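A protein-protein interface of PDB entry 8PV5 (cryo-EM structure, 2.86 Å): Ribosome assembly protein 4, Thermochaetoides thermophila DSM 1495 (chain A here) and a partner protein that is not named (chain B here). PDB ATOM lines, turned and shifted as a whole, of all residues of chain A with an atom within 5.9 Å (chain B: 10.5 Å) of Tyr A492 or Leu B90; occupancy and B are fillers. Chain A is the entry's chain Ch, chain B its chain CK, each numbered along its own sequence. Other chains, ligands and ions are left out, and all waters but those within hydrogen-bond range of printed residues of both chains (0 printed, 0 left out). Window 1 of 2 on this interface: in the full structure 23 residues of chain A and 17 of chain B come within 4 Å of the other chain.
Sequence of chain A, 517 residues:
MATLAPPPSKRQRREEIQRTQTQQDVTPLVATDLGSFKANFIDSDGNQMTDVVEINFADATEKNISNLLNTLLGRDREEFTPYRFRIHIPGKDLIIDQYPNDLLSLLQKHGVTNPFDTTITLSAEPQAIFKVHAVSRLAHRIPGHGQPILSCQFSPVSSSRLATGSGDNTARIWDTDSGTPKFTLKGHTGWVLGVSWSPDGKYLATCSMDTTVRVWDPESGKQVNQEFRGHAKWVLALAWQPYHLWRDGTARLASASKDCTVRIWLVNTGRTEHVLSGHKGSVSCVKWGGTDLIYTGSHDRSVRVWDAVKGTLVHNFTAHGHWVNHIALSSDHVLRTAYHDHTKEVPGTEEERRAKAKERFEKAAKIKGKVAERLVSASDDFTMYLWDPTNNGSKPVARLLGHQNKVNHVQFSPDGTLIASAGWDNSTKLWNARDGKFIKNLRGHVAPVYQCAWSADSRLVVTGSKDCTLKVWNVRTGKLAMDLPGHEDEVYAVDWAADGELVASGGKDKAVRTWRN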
ATOM      1  N   PRO A 148       2.374  21.530  -2.796  1.00  0.00           N
ATOM      2  CA  PRO A 148       3.252  21.730  -1.634  1.00  0.00           C
ATOM      3  C   PRO A 148       2.863  22.929  -0.778  1.00  0.00           C
ATOM      4  O   PRO A 148       2.432  23.967  -1.281  1.00  0.00           O
ATOM      5  CB  PRO A 148       4.627  21.934  -2.273  1.00  0.00           C
ATOM      6  CG  PRO A 148       4.575  21.102  -3.482  1.00  0.00           C
ATOM      7  CD  PRO A 148       3.163  21.197  -3.999  1.00  0.00           C
ATOM      8  N   ILE A 149       3.025  22.762   0.533  1.00  0.00           N
ATOM      9  CA  ILE A 149       2.623  23.783   1.491  1.00  0.00           C
ATOM     10  C   ILE A 149       3.752  24.788   1.661  1.00  0.00           C
ATOM     11  O   ILE A 149       4.900  24.416   1.937  1.00  0.00           O
ATOM     12  CB  ILE A 149       2.250  23.131   2.828  1.00  0.00           C
ATOM     13  CG1 ILE A 149       1.184  22.063   2.599  1.00  0.00           C
ATOM     14  CG2 ILE A 149       1.766  24.175   3.819  1.00  0.00           C
ATOM     15  CD1 ILE A 149       0.960  21.174   3.777  1.00  0.00           C
ATOM     16  N   LEU A 150       3.430  26.071   1.507  1.00  0.00           N
ATOM     17  CA  LEU A 150       4.438  27.118   1.520  1.00  0.00           C
ATOM     18  C   LEU A 150       4.513  27.900   2.822  1.00  0.00           C
ATOM     19  O   LEU A 150       5.581  28.446   3.124  1.00  0.00           O
ATOM     20  CB  LEU A 150       4.200  28.099   0.363  1.00  0.00           C
ATOM     21  CG  LEU A 150       3.963  27.440  -0.995  1.00  0.00           C
ATOM     22  CD1 LEU A 150       3.639  28.486  -2.040  1.00  0.00           C
ATOM     23  CD2 LEU A 150       5.171  26.620  -1.411  1.00  0.00           C
ATOM     24  N   ASN A 408      19.454  31.424   5.646  1.00  0.00           N
ATOM     25  CA  ASN A 408      18.076  31.508   5.184  1.00  0.00           C
ATOM     26  C   ASN A 408      17.144  32.149   6.203  1.00  0.00           C
ATOM     27  O   ASN A 408      16.318  32.992   5.839  1.00  0.00           O
ATOM     28  CB  ASN A 408      17.561  30.114   4.827  1.00  0.00           C
ATOM     29  CG  ASN A 408      16.386  30.156   3.879  1.00  0.00           C
ATOM     30  OD1 ASN A 408      16.511  30.597   2.739  1.00  0.00           O
ATOM     31  ND2 ASN A 408      15.234  29.695   4.346  1.00  0.00           N
ATOM     32  N   TRP A 424      22.571  27.456   4.721  1.00  0.00           N
ATOM     33  CA  TRP A 424      22.652  26.501   3.626  1.00  0.00           C
ATOM     34  C   TRP A 424      23.885  25.616   3.719  1.00  0.00           C
ATOM     35  O   TRP A 424      24.077  24.750   2.861  1.00  0.00           O
ATOM     36  CB  TRP A 424      22.637  27.236   2.283  1.00  0.00           C
ATOM     37  CG  TRP A 424      21.291  27.771   1.893  1.00  0.00           C
ATOM     38  CD1 TRP A 424      20.502  28.613   2.617  1.00  0.00           C
ATOM     39  CD2 TRP A 424      20.586  27.509   0.676  1.00  0.00           C
ATOM     40  NE1 TRP A 424      19.346  28.887   1.931  1.00  0.00           N
ATOM     41  CE2 TRP A 424      19.373  28.221   0.734  1.00  0.00           C
ATOM     42  CE3 TRP A 424      20.861  26.739  -0.457  1.00  0.00           C
ATOM     43  CZ2 TRP A 424      18.436  28.186  -0.294  1.00  0.00           C
ATOM     44  CZ3 TRP A 424      19.930  26.705  -1.477  1.00  0.00           C
ATOM     45  CH2 TRP A 424      18.734  27.423  -1.389  1.00  0.00           C
ATOM     46  N   TYR A 450      16.154  25.085   6.216  1.00  0.00           N
ATOM     47  CA  TYR A 450      15.305  26.144   5.694  1.00  0.00           C
ATOM     48  C   TYR A 450      14.659  26.992   6.777  1.00  0.00           C
ATOM     49  O   TYR A 450      14.604  28.218   6.628  1.00  0.00           O
ATOM     50  CB  TYR A 450      14.223  25.564   4.781  1.00  0.00           C
ATOM     51  CG  TYR A 450      14.735  25.184   3.413  1.00  0.00           C
ATOM     52  CD1 TYR A 450      15.741  25.918   2.803  1.00  0.00           C
ATOM     53  CD2 TYR A 450      14.203  24.103   2.725  1.00  0.00           C
ATOM     54  CE1 TYR A 450      16.212  25.581   1.553  1.00  0.00           C
ATOM     55  CE2 TYR A 450      14.667  23.759   1.472  1.00  0.00           C
ATOM     56  CZ  TYR A 450      15.672  24.501   0.891  1.00  0.00           C
ATOM     57  OH  TYR A 450      16.140  24.164  -0.356  1.00  0.00           O
ATOM     58  N   GLN A 451      14.163  26.399   7.862  1.00  0.00           N
ATOM     59  CA  GLN A 451      13.495  27.230   8.855  1.00  0.00           C
ATOM     60  C   GLN A 451      13.887  26.814  10.263  1.00  0.00           C
ATOM     61  O   GLN A 451      14.268  25.671  10.515  1.00  0.00           O
ATOM     62  CB  GLN A 451      11.971  27.186   8.706  1.00  0.00           C
ATOM     63  CG  GLN A 451      11.435  28.117   7.637  1.00  0.00           C
ATOM     64  CD  GLN A 451      10.089  28.694   8.001  1.00  0.00           C
ATOM     65  OE1 GLN A 451       9.715  28.729   9.172  1.00  0.00           O
ATOM     66  NE2 GLN A 451       9.349  29.150   6.999  1.00  0.00           N
ATOM     67  N   SER A 465      14.471  21.142   7.725  1.00  0.00           N
ATOM     68  CA  SER A 465      15.441  21.251   6.644  1.00  0.00           C
ATOM     69  C   SER A 465      14.961  20.552   5.379  1.00  0.00           C
ATOM     70  O   SER A 465      13.878  19.966   5.322  1.00  0.00           O
ATOM     71  CB  SER A 465      16.797  20.674   7.064  1.00  0.00           C
ATOM     72  OG  SER A 465      17.679  20.597   5.959  1.00  0.00           O
ATOM     73  N   GLU A 490      10.751  17.545   1.043  1.00  0.00           N
ATOM     74  CA  GLU A 490      11.381  18.667   1.731  1.00  0.00           C
ATOM     75  C   GLU A 490      10.405  19.377   2.661  1.00  0.00           C
ATOM     76  O   GLU A 490       9.194  19.384   2.434  1.00  0.00           O
ATOM     77  CB  GLU A 490      11.935  19.669   0.719  1.00  0.00           C
ATOM     78  CG  GLU A 490      12.809  19.066  -0.358  1.00  0.00           C
ATOM     79  CD  GLU A 490      13.374  20.118  -1.289  1.00  0.00           C
ATOM     80  OE1 GLU A 490      13.369  21.307  -0.913  1.00  0.00           O
ATOM     81  OE2 GLU A 490      13.818  19.756  -2.399  1.00  0.00           O
ATOM     82  N   VAL A 491      10.949  19.975   3.715  1.00  0.00           N
ATOM     83  CA  VAL A 491      10.163  20.735   4.678  1.00  0.00           C
ATOM     84  C   VAL A 491      10.348  22.218   4.389  1.00  0.00           C
ATOM     85  O   VAL A 491      11.479  22.716   4.350  1.00  0.00           O
ATOM     86  CB  VAL A 491      10.584  20.396   6.117  1.00  0.00           C
ATOM     87  CG1 VAL A 491       9.775  21.206   7.108  1.00  0.00           C
ATOM     88  CG2 VAL A 491      10.426  18.911   6.377  1.00  0.00           C
ATOM     89  N   TYR A 492       9.239  22.925   4.187  1.00  0.00           N
ATOM     90  CA  TYR A 492       9.279  24.338   3.836  1.00  0.00           C
ATOM     91  C   TYR A 492       8.959  25.273   4.989  1.00  0.00           C
ATOM     92  O   TYR A 492       9.655  26.276   5.160  1.00  0.00           O
ATOM     93  CB  TYR A 492       8.308  24.631   2.688  1.00  0.00           C
ATOM     94  CG  TYR A 492       8.783  24.146   1.338  1.00  0.00           C
ATOM     95  CD1 TYR A 492      10.131  24.147   1.014  1.00  0.00           C
ATOM     96  CD2 TYR A 492       7.879  23.699   0.384  1.00  0.00           C
ATOM     97  CE1 TYR A 492      10.568  23.709  -0.221  1.00  0.00           C
ATOM     98  CE2 TYR A 492       8.306  23.259  -0.852  1.00  0.00           C
ATOM     99  CZ  TYR A 492       9.651  23.265  -1.148  1.00  0.00           C
ATOM    100  OH  TYR A 492      10.079  22.828  -2.378  1.00  0.00           O
ATOM    101  N   ALA A 493       7.930  24.980   5.780  1.00  0.00           N
ATOM    102  CA  ALA A 493       7.480  25.873   6.835  1.00  0.00           C
ATOM    103  C   ALA A 493       7.427  25.134   8.163  1.00  0.00           C
ATOM    104  O   ALA A 493       6.863  24.039   8.251  1.00  0.00           O
ATOM    105  CB  ALA A 493       6.107  26.460   6.508  1.00  0.00           C
ATOM    106  N   VAL A 494       8.019  25.741   9.191  1.00  0.00           N
ATOM    107  CA  VAL A 494       8.057  25.186  10.541  1.00  0.00           C
ATOM    108  C   VAL A 494       7.614  26.263  11.522  1.00  0.00           C
ATOM    109  O   VAL A 494       8.130  27.385  11.500  1.00  0.00           O
ATOM    110  CB  VAL A 494       9.466  24.667  10.903  1.00  0.00           C
ATOM    111  CG1 VAL A 494       9.548  24.311  12.374  1.00  0.00           C
ATOM    112  CG2 VAL A 494       9.818  23.463  10.062  1.00  0.00           C
ATOM    113  N   GLY A 506       5.190  21.847   7.324  1.00  0.00           N
ATOM    114  CA  GLY A 506       4.619  21.607   6.013  1.00  0.00           C
ATOM    115  C   GLY A 506       5.694  21.749   4.964  1.00  0.00           C
ATOM    116  O   GLY A 506       6.705  22.426   5.176  1.00  0.00           O
ATOM    117  N   GLY A 507       5.477  21.107   3.824  1.00  0.00           N
ATOM    118  CA  GLY A 507       6.454  21.186   2.761  1.00  0.00           C
ATOM    119  C   GLY A 507       6.012  20.560   1.459  1.00  0.00           C
ATOM    120  O   GLY A 507       4.843  20.649   1.077  1.00  0.00           O
ATOM    121  N   LYS A 508       6.951  19.910   0.775  1.00  0.00           N
ATOM    122  CA  LYS A 508       6.700  19.364  -0.551  1.00  0.00           C
ATOM    123  C   LYS A 508       5.864  18.088  -0.527  1.00  0.00           C
ATOM    124  O   LYS A 508       5.400  17.651  -1.585  1.00  0.00           O
ATOM    125  CB  LYS A 508       8.036  19.106  -1.250  1.00  0.00           C
ATOM    126  CG  LYS A 508       8.020  19.251  -2.756  1.00  0.00           C
ATOM    127  CD  LYS A 508       9.428  19.131  -3.309  1.00  0.00           C
ATOM    128  CE  LYS A 508       9.425  19.019  -4.820  1.00  0.00           C
ATOM    129  NZ  LYS A 508      10.791  18.765  -5.349  1.00  0.00           N
ATOM    130  N   PRO B  82       7.414  30.299 -11.725  1.00  0.00           N
ATOM    131  CA  PRO B  82       7.909  28.922 -11.838  1.00  0.00           C
ATOM    132  C   PRO B  82       6.772  27.917 -11.980  1.00  0.00           C
ATOM    133  O   PRO B  82       5.605  28.306 -11.998  1.00  0.00           O
ATOM    134  CB  PRO B  82       8.670  28.692 -10.527  1.00  0.00           C
ATOM    135  CG  PRO B  82       8.767  30.002  -9.846  1.00  0.00           C
ATOM    136  CD  PRO B  82       7.962  31.025 -10.567  1.00  0.00           C
ATOM    137  N   SER B  83       7.116  26.634 -12.082  1.00  0.00           N
ATOM    138  CA  SER B  83       6.109  25.586 -12.202  1.00  0.00           C
ATOM    139  C   SER B  83       5.869  24.916 -10.855  1.00  0.00           C
ATOM    140  O   SER B  83       4.728  24.841 -10.387  1.00  0.00           O
ATOM    141  CB  SER B  83       6.535  24.552 -13.246  1.00  0.00           C
ATOM    142  OG  SER B  83       6.716  25.153 -14.515  1.00  0.00           O
ATOM    143  N   ASP B  84       6.935  24.424 -10.231  1.00  0.00           N
ATOM    144  CA  ASP B  84       6.837  23.786  -8.925  1.00  0.00           C
ATOM    145  C   ASP B  84       6.650  24.846  -7.840  1.00  0.00           C
ATOM    146  O   ASP B  84       7.410  25.817  -7.789  1.00  0.00           O
ATOM    147  CB  ASP B  84       8.092  22.965  -8.640  1.00  0.00           C
ATOM    148  CG  ASP B  84       7.821  21.767  -7.750  1.00  0.00           C
ATOM    149  OD1 ASP B  84       6.641  21.489  -7.455  1.00  0.00           O
ATOM    150  OD2 ASP B  84       8.794  21.099  -7.343  1.00  0.00           O
ATOM    151  N   PRO B  85       5.630  24.703  -6.989  1.00  0.00           N
ATOM    152  CA  PRO B  85       5.436  25.660  -5.891  1.00  0.00           C
ATOM    153  C   PRO B  85       6.609  25.680  -4.920  1.00  0.00           C
ATOM    154  O   PRO B  85       6.994  24.655  -4.355  1.00  0.00           O
ATOM    155  CB  PRO B  85       4.156  25.158  -5.218  1.00  0.00           C
ATOM    156  CG  PRO B  85       3.401  24.522  -6.320  1.00  0.00           C
ATOM    157  CD  PRO B  85       4.434  23.871  -7.203  1.00  0.00           C
ATOM    158  N   ILE B  86       7.174  26.869  -4.733  1.00  0.00           N
ATOM    159  CA  ILE B  86       8.305  27.081  -3.834  1.00  0.00           C
ATOM    160  C   ILE B  86       7.991  28.283  -2.954  1.00  0.00           C
ATOM    161  O   ILE B  86       7.224  29.174  -3.351  1.00  0.00           O
ATOM    162  CB  ILE B  86       9.625  27.292  -4.616  1.00  0.00           C
ATOM    163  CG1 ILE B  86       9.453  28.381  -5.674  1.00  0.00           C
ATOM    164  CG2 ILE B  86      10.096  25.992  -5.246  1.00  0.00           C
ATOM    165  CD1 ILE B  86      10.725  28.719  -6.410  1.00  0.00           C
ATOM    166  N   PRO B  87       8.551  28.333  -1.746  1.00  0.00           N
ATOM    167  CA  PRO B  87       8.292  29.478  -0.866  1.00  0.00           C
ATOM    168  C   PRO B  87       8.981  30.750  -1.342  1.00  0.00           C
ATOM    169  O   PRO B  87       9.748  30.765  -2.310  1.00  0.00           O
ATOM    170  CB  PRO B  87       8.848  29.030   0.490  1.00  0.00           C
ATOM    171  CG  PRO B  87       8.994  27.565   0.396  1.00  0.00           C
ATOM    172  CD  PRO B  87       9.241  27.244  -1.034  1.00  0.00           C
ATOM    173  N   SER B  88       8.686  31.835  -0.623  1.00  0.00           N
ATOM    174  CA  SER B  88       9.173  33.154  -1.007  1.00  0.00           C
ATOM    175  C   SER B  88      10.683  33.273  -0.857  1.00  0.00           C
ATOM    176  O   SER B  88      11.327  33.986  -1.634  1.00  0.00           O
ATOM    177  CB  SER B  88       8.472  34.228  -0.178  1.00  0.00           C
ATOM    178  OG  SER B  88       8.787  34.092   1.196  1.00  0.00           O
ATOM    179  N   TYR B  89      11.268  32.593   0.131  1.00  0.00           N
ATOM    180  CA  TYR B  89      12.718  32.618   0.272  1.00  0.00           C
ATOM    181  C   TYR B  89      13.421  31.775  -0.783  1.00  0.00           C
ATOM    182  O   TYR B  89      14.631  31.938  -0.974  1.00  0.00           O
ATOM    183  CB  TYR B  89      13.128  32.168   1.679  1.00  0.00           C
ATOM    184  CG  TYR B  89      12.543  30.847   2.136  1.00  0.00           C
ATOM    185  CD1 TYR B  89      13.115  29.639   1.757  1.00  0.00           C
ATOM    186  CD2 TYR B  89      11.430  30.810   2.964  1.00  0.00           C
ATOM    187  CE1 TYR B  89      12.587  28.434   2.176  1.00  0.00           C
ATOM    188  CE2 TYR B  89      10.897  29.610   3.390  1.00  0.00           C
ATOM    189  CZ  TYR B  89      11.480  28.426   2.993  1.00  0.00           C
ATOM    190  OH  TYR B  89      10.955  27.227   3.412  1.00  0.00           O
ATOM    191  N   LEU B  90      12.703  30.884  -1.463  1.00  0.00           N
ATOM    192  CA  LEU B  90      13.248  30.122  -2.576  1.00  0.00           C
ATOM    193  C   LEU B  90      12.885  30.715  -3.928  1.00  0.00           C
ATOM    194  O   LEU B  90      13.401  30.252  -4.949  1.00  0.00           O
ATOM    195  CB  LEU B  90      12.772  28.668  -2.510  1.00  0.00           C
ATOM    196  CG  LEU B  90      13.355  27.815  -1.386  1.00  0.00           C
ATOM    197  CD1 LEU B  90      12.861  26.388  -1.499  1.00  0.00           C
ATOM    198  CD2 LEU B  90      14.871  27.866  -1.406  1.00  0.00           C
ATOM    199  N   LEU B  91      11.999  31.708  -3.961  1.00  0.00           N
ATOM    200  CA  LEU B  91      11.700  32.405  -5.204  1.00  0.00           C
ATOM    201  C   LEU B  91      12.911  33.193  -5.691  1.00  0.00           C
ATOM    202  O   LEU B  91      13.780  33.586  -4.907  1.00  0.00           O
ATOM    203  CB  LEU B  91      10.510  33.347  -5.023  1.00  0.00           C
ATOM    204  CG  LEU B  91       9.130  32.697  -4.956  1.00  0.00           C
ATOM    205  CD1 LEU B  91       8.067  33.732  -4.642  1.00  0.00           C
ATOM    206  CD2 LEU B  91       8.825  31.990  -6.260  1.00  0.00           C
ATOM    207  N   ASP B  92      12.968  33.394  -7.010  1.00  0.00           N
ATOM    208  CA  ASP B  92      13.992  34.127  -7.757  1.00  0.00           C
ATOM    209  C   ASP B  92      15.375  33.489  -7.685  1.00  0.00           C
ATOM    210  O   ASP B  92      16.354  34.138  -8.069  1.00  0.00           O
ATOM    211  CB  ASP B  92      14.110  35.596  -7.323  1.00  0.00           C
ATOM    212  CG  ASP B  92      12.901  36.418  -7.708  1.00  0.00           C
ATOM    213  OD1 ASP B  92      12.256  36.086  -8.724  1.00  0.00           O
ATOM    214  OD2 ASP B  92      12.591  37.392  -6.991  1.00  0.00           O
ATOM    215  N   ARG B  93      15.495  32.253  -7.218  1.00  0.00           N
ATOM    216  CA  ARG B  93      16.768  31.553  -7.189  1.00  0.00           C
ATOM    217  C   ARG B  93      16.854  30.560  -8.341  1.00  0.00           C
ATOM    218  O   ARG B  93      15.858  30.240  -8.993  1.00  0.00           O
ATOM    219  CB  ARG B  93      16.964  30.822  -5.859  1.00  0.00           C
ATOM    220  CG  ARG B  93      16.895  31.711  -4.635  1.00  0.00           C
ATOM    221  CD  ARG B  93      17.248  30.929  -3.385  1.00  0.00           C
ATOM    222  NE  ARG B  93      17.269  31.772  -2.196  1.00  0.00           N
ATOM    223  CZ  ARG B  93      18.307  32.503  -1.813  1.00  0.00           C
ATOM    224  NH1 ARG B  93      19.431  32.524  -2.508  1.00  0.00           N
ATOM    225  NH2 ARG B  93      18.214  33.229  -0.704  1.00  0.00           N
ATOM    226  N   ALA B  94      18.068  30.078  -8.586  1.00  0.00           N
ATOM    227  CA  ALA B  94      18.285  29.047  -9.594  1.00  0.00           C
ATOM    228  C   ALA B  94      17.873  27.698  -9.019  1.00  0.00           C
ATOM    229  O   ALA B  94      18.601  27.108  -8.215  1.00  0.00           O
ATOM    230  CB  ALA B  94      19.745  29.035 -10.034  1.00  0.00           C
ATOM    231  N   ASN B  95      16.706  27.208  -9.428  1.00  0.00           N
ATOM    232  CA  ASN B  95      16.166  25.960  -8.927  1.00  0.00           C
ATOM    233  C   ASN B  95      16.223  24.899 -10.017  1.00  0.00           C
ATOM    234  O   ASN B  95      16.148  25.241 -11.208  1.00  0.00           O
ATOM    235  CB  ASN B  95      14.713  26.145  -8.450  1.00  0.00           C
ATOM    236  CG  ASN B  95      14.626  26.822  -7.097  1.00  0.00           C
ATOM    237  OD1 ASN B  95      14.608  28.049  -7.002  1.00  0.00           O
ATOM    238  ND2 ASN B  95      14.570  26.024  -6.038  1.00  0.00           N
ATOM    239  N   PRO B  96      16.379  23.623  -9.666  1.00  0.00           N
ATOM    240  CA  PRO B  96      16.362  22.567 -10.684  1.00  0.00           C
ATOM    241  C   PRO B  96      14.995  22.448 -11.343  1.00  0.00           C
ATOM    242  O   PRO B  96      13.965  22.764 -10.743  1.00  0.00           O
ATOM    243  CB  PRO B  96      16.718  21.305  -9.891  1.00  0.00           C
ATOM    244  CG  PRO B  96      17.423  21.800  -8.674  1.00  0.00           C
ATOM    245  CD  PRO B  96      16.780  23.111  -8.344  1.00  0.00           C
ATOM    246  N   THR B  98      13.514  19.639 -12.306  1.00  0.00           N
ATOM    247  CA  THR B  98      12.848  18.484 -11.688  1.00  0.00           C
ATOM    248  C   THR B  98      11.776  17.911 -12.622  1.00  0.00           C
ATOM    249  O   THR B  98      10.573  18.018 -12.365  1.00  0.00           O
ATOM    250  CB  THR B  98      12.279  18.833 -10.304  1.00  0.00           C
ATOM    251  OG1 THR B  98      13.303  19.462  -9.527  1.00  0.00           O
ATOM    252  CG2 THR B  98      11.869  17.567  -9.544  1.00  0.00           C
ATOM    253  N   LEU B 189      15.814  14.235  -8.094  1.00  0.00           N
ATOM    254  CA  LEU B 189      16.181  15.606  -7.762  1.00  0.00           C
ATOM    255  C   LEU B 189      16.747  16.369  -8.952  1.00  0.00           C
ATOM    256  O   LEU B 189      16.824  17.601  -8.887  1.00  0.00           O
ATOM    257  CB  LEU B 189      17.192  15.618  -6.615  1.00  0.00           C
ATOM    258  CG  LEU B 189      16.907  14.688  -5.436  1.00  0.00           C
ATOM    259  CD1 LEU B 189      18.063  14.707  -4.451  1.00  0.00           C
ATOM    260  CD2 LEU B 189      15.606  15.069  -4.750  1.00  0.00           C
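Hydrophobic or aromatic side chains of chain A that line the printed part of chain B: Leu A150, Trp A424, Tyr A450 and Tyr A492.
Among the printed residues, Asp or Glu carboxylates within 4 Å of a Lys or Arg side-chain nitrogen of the other chain: Lys A508 with Asp B84.
Of the printed residues of chain B, Leu A150 touches Pro B85 (3.9 Å), Ile B86 (3.6 Å) and Pro B87 (3.8 Å).
Printed residues of chain B within 4 Å of Asn A408: Tyr B89.
Of the printed residues of chain B, Gln A451 touches Tyr B89 (3.95 Å).
No residue of chain B comes within 4 Å of Val A491.
Printed residues of chain B within 4 Å of Tyr A492: Pro B85, Pro B87, Tyr B89 and Leu B90.
No residue of chain B comes within 4 Å of Ala A493.
No residue of chain B comes within 4 Å of Gly A506.
No residue of chain B comes within 4 Å of Gly A507.
Lys A508 touches just one residue of chain B: Asp B84.
Ser B83 touches none of the printed residues of chain A.
Printed residues of chain A within 4 Å of Asp B84: Lys A508.
Printed residues of chain A within 4 Å of Pro B87: Leu A150 and Tyr A492.
Leu B90 touches three residues of chain A.
The nearest printed residue of chain B that does not touch Tyr A492 is Ile B86 (4.3 Å).
The nearest printed residue of chain A that does not touch Asp B84 is Pro A148 (4.5 Å).
The side-chain amino group (NZ) of Lys A508 lies within salt-bridge range of the side-chain carboxylate (OD2) of Asp B84 (3.7 Å).
The side-chain hydroxyl of Tyr B89 sits close to the backbone carbonyl oxygen of Tyr A492 (2.4 Å).
Leu A150 touches Pro B85 (CD2 to C, 3.9 Å).
Ile B86 touches Leu A150 (C to CD2, 3.6 Å).
Pro B87 touches Leu A150 (N to CD2, 3.8 Å).
ND2 of Asn A408 touches CD1 of Tyr B89, at 3.3 Å.
CD2 of Leu B90 touches CZ2 of Trp A424, at 3.7 Å.
Tyr B89 touches Tyr A450 (OH to CB, 3.9 Å).
Tyr A450 touches Leu B90.
Gln A451 touches Tyr B89 (NE2 to CE2, 3.95 Å).
Tyr A492 touches Pro B85.
Tyr A492 touches Leu B90.
The indole nitrogen of Trp A424 is in hydrogen-bond range of the side-chain amide oxygen of Asn A408.
O of Tyr A450 lies within hydrogen-bond range of ND2 of Asn A408.
The side-chain amide oxygen (OE1) of Gln A451 sits close to the backbone carbonyl oxygen (O) of Val A494 (3.1 Å).
The backbone carbonyl oxygen (O) of Glu A490 sits at hydrogen-bond distance from the backbone NH (N) of Lys A508 (2.8 Å).
The backbone NH (N) of Tyr A492 lies within hydrogen-bond range of the backbone carbonyl oxygen (O) of Gly A506 (2.8 Å).
The guanidinium group (NE) of Arg B93 sits at hydrogen-bond distance from the backbone carbonyl oxygen (O) of Tyr B89 (2.9 Å).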
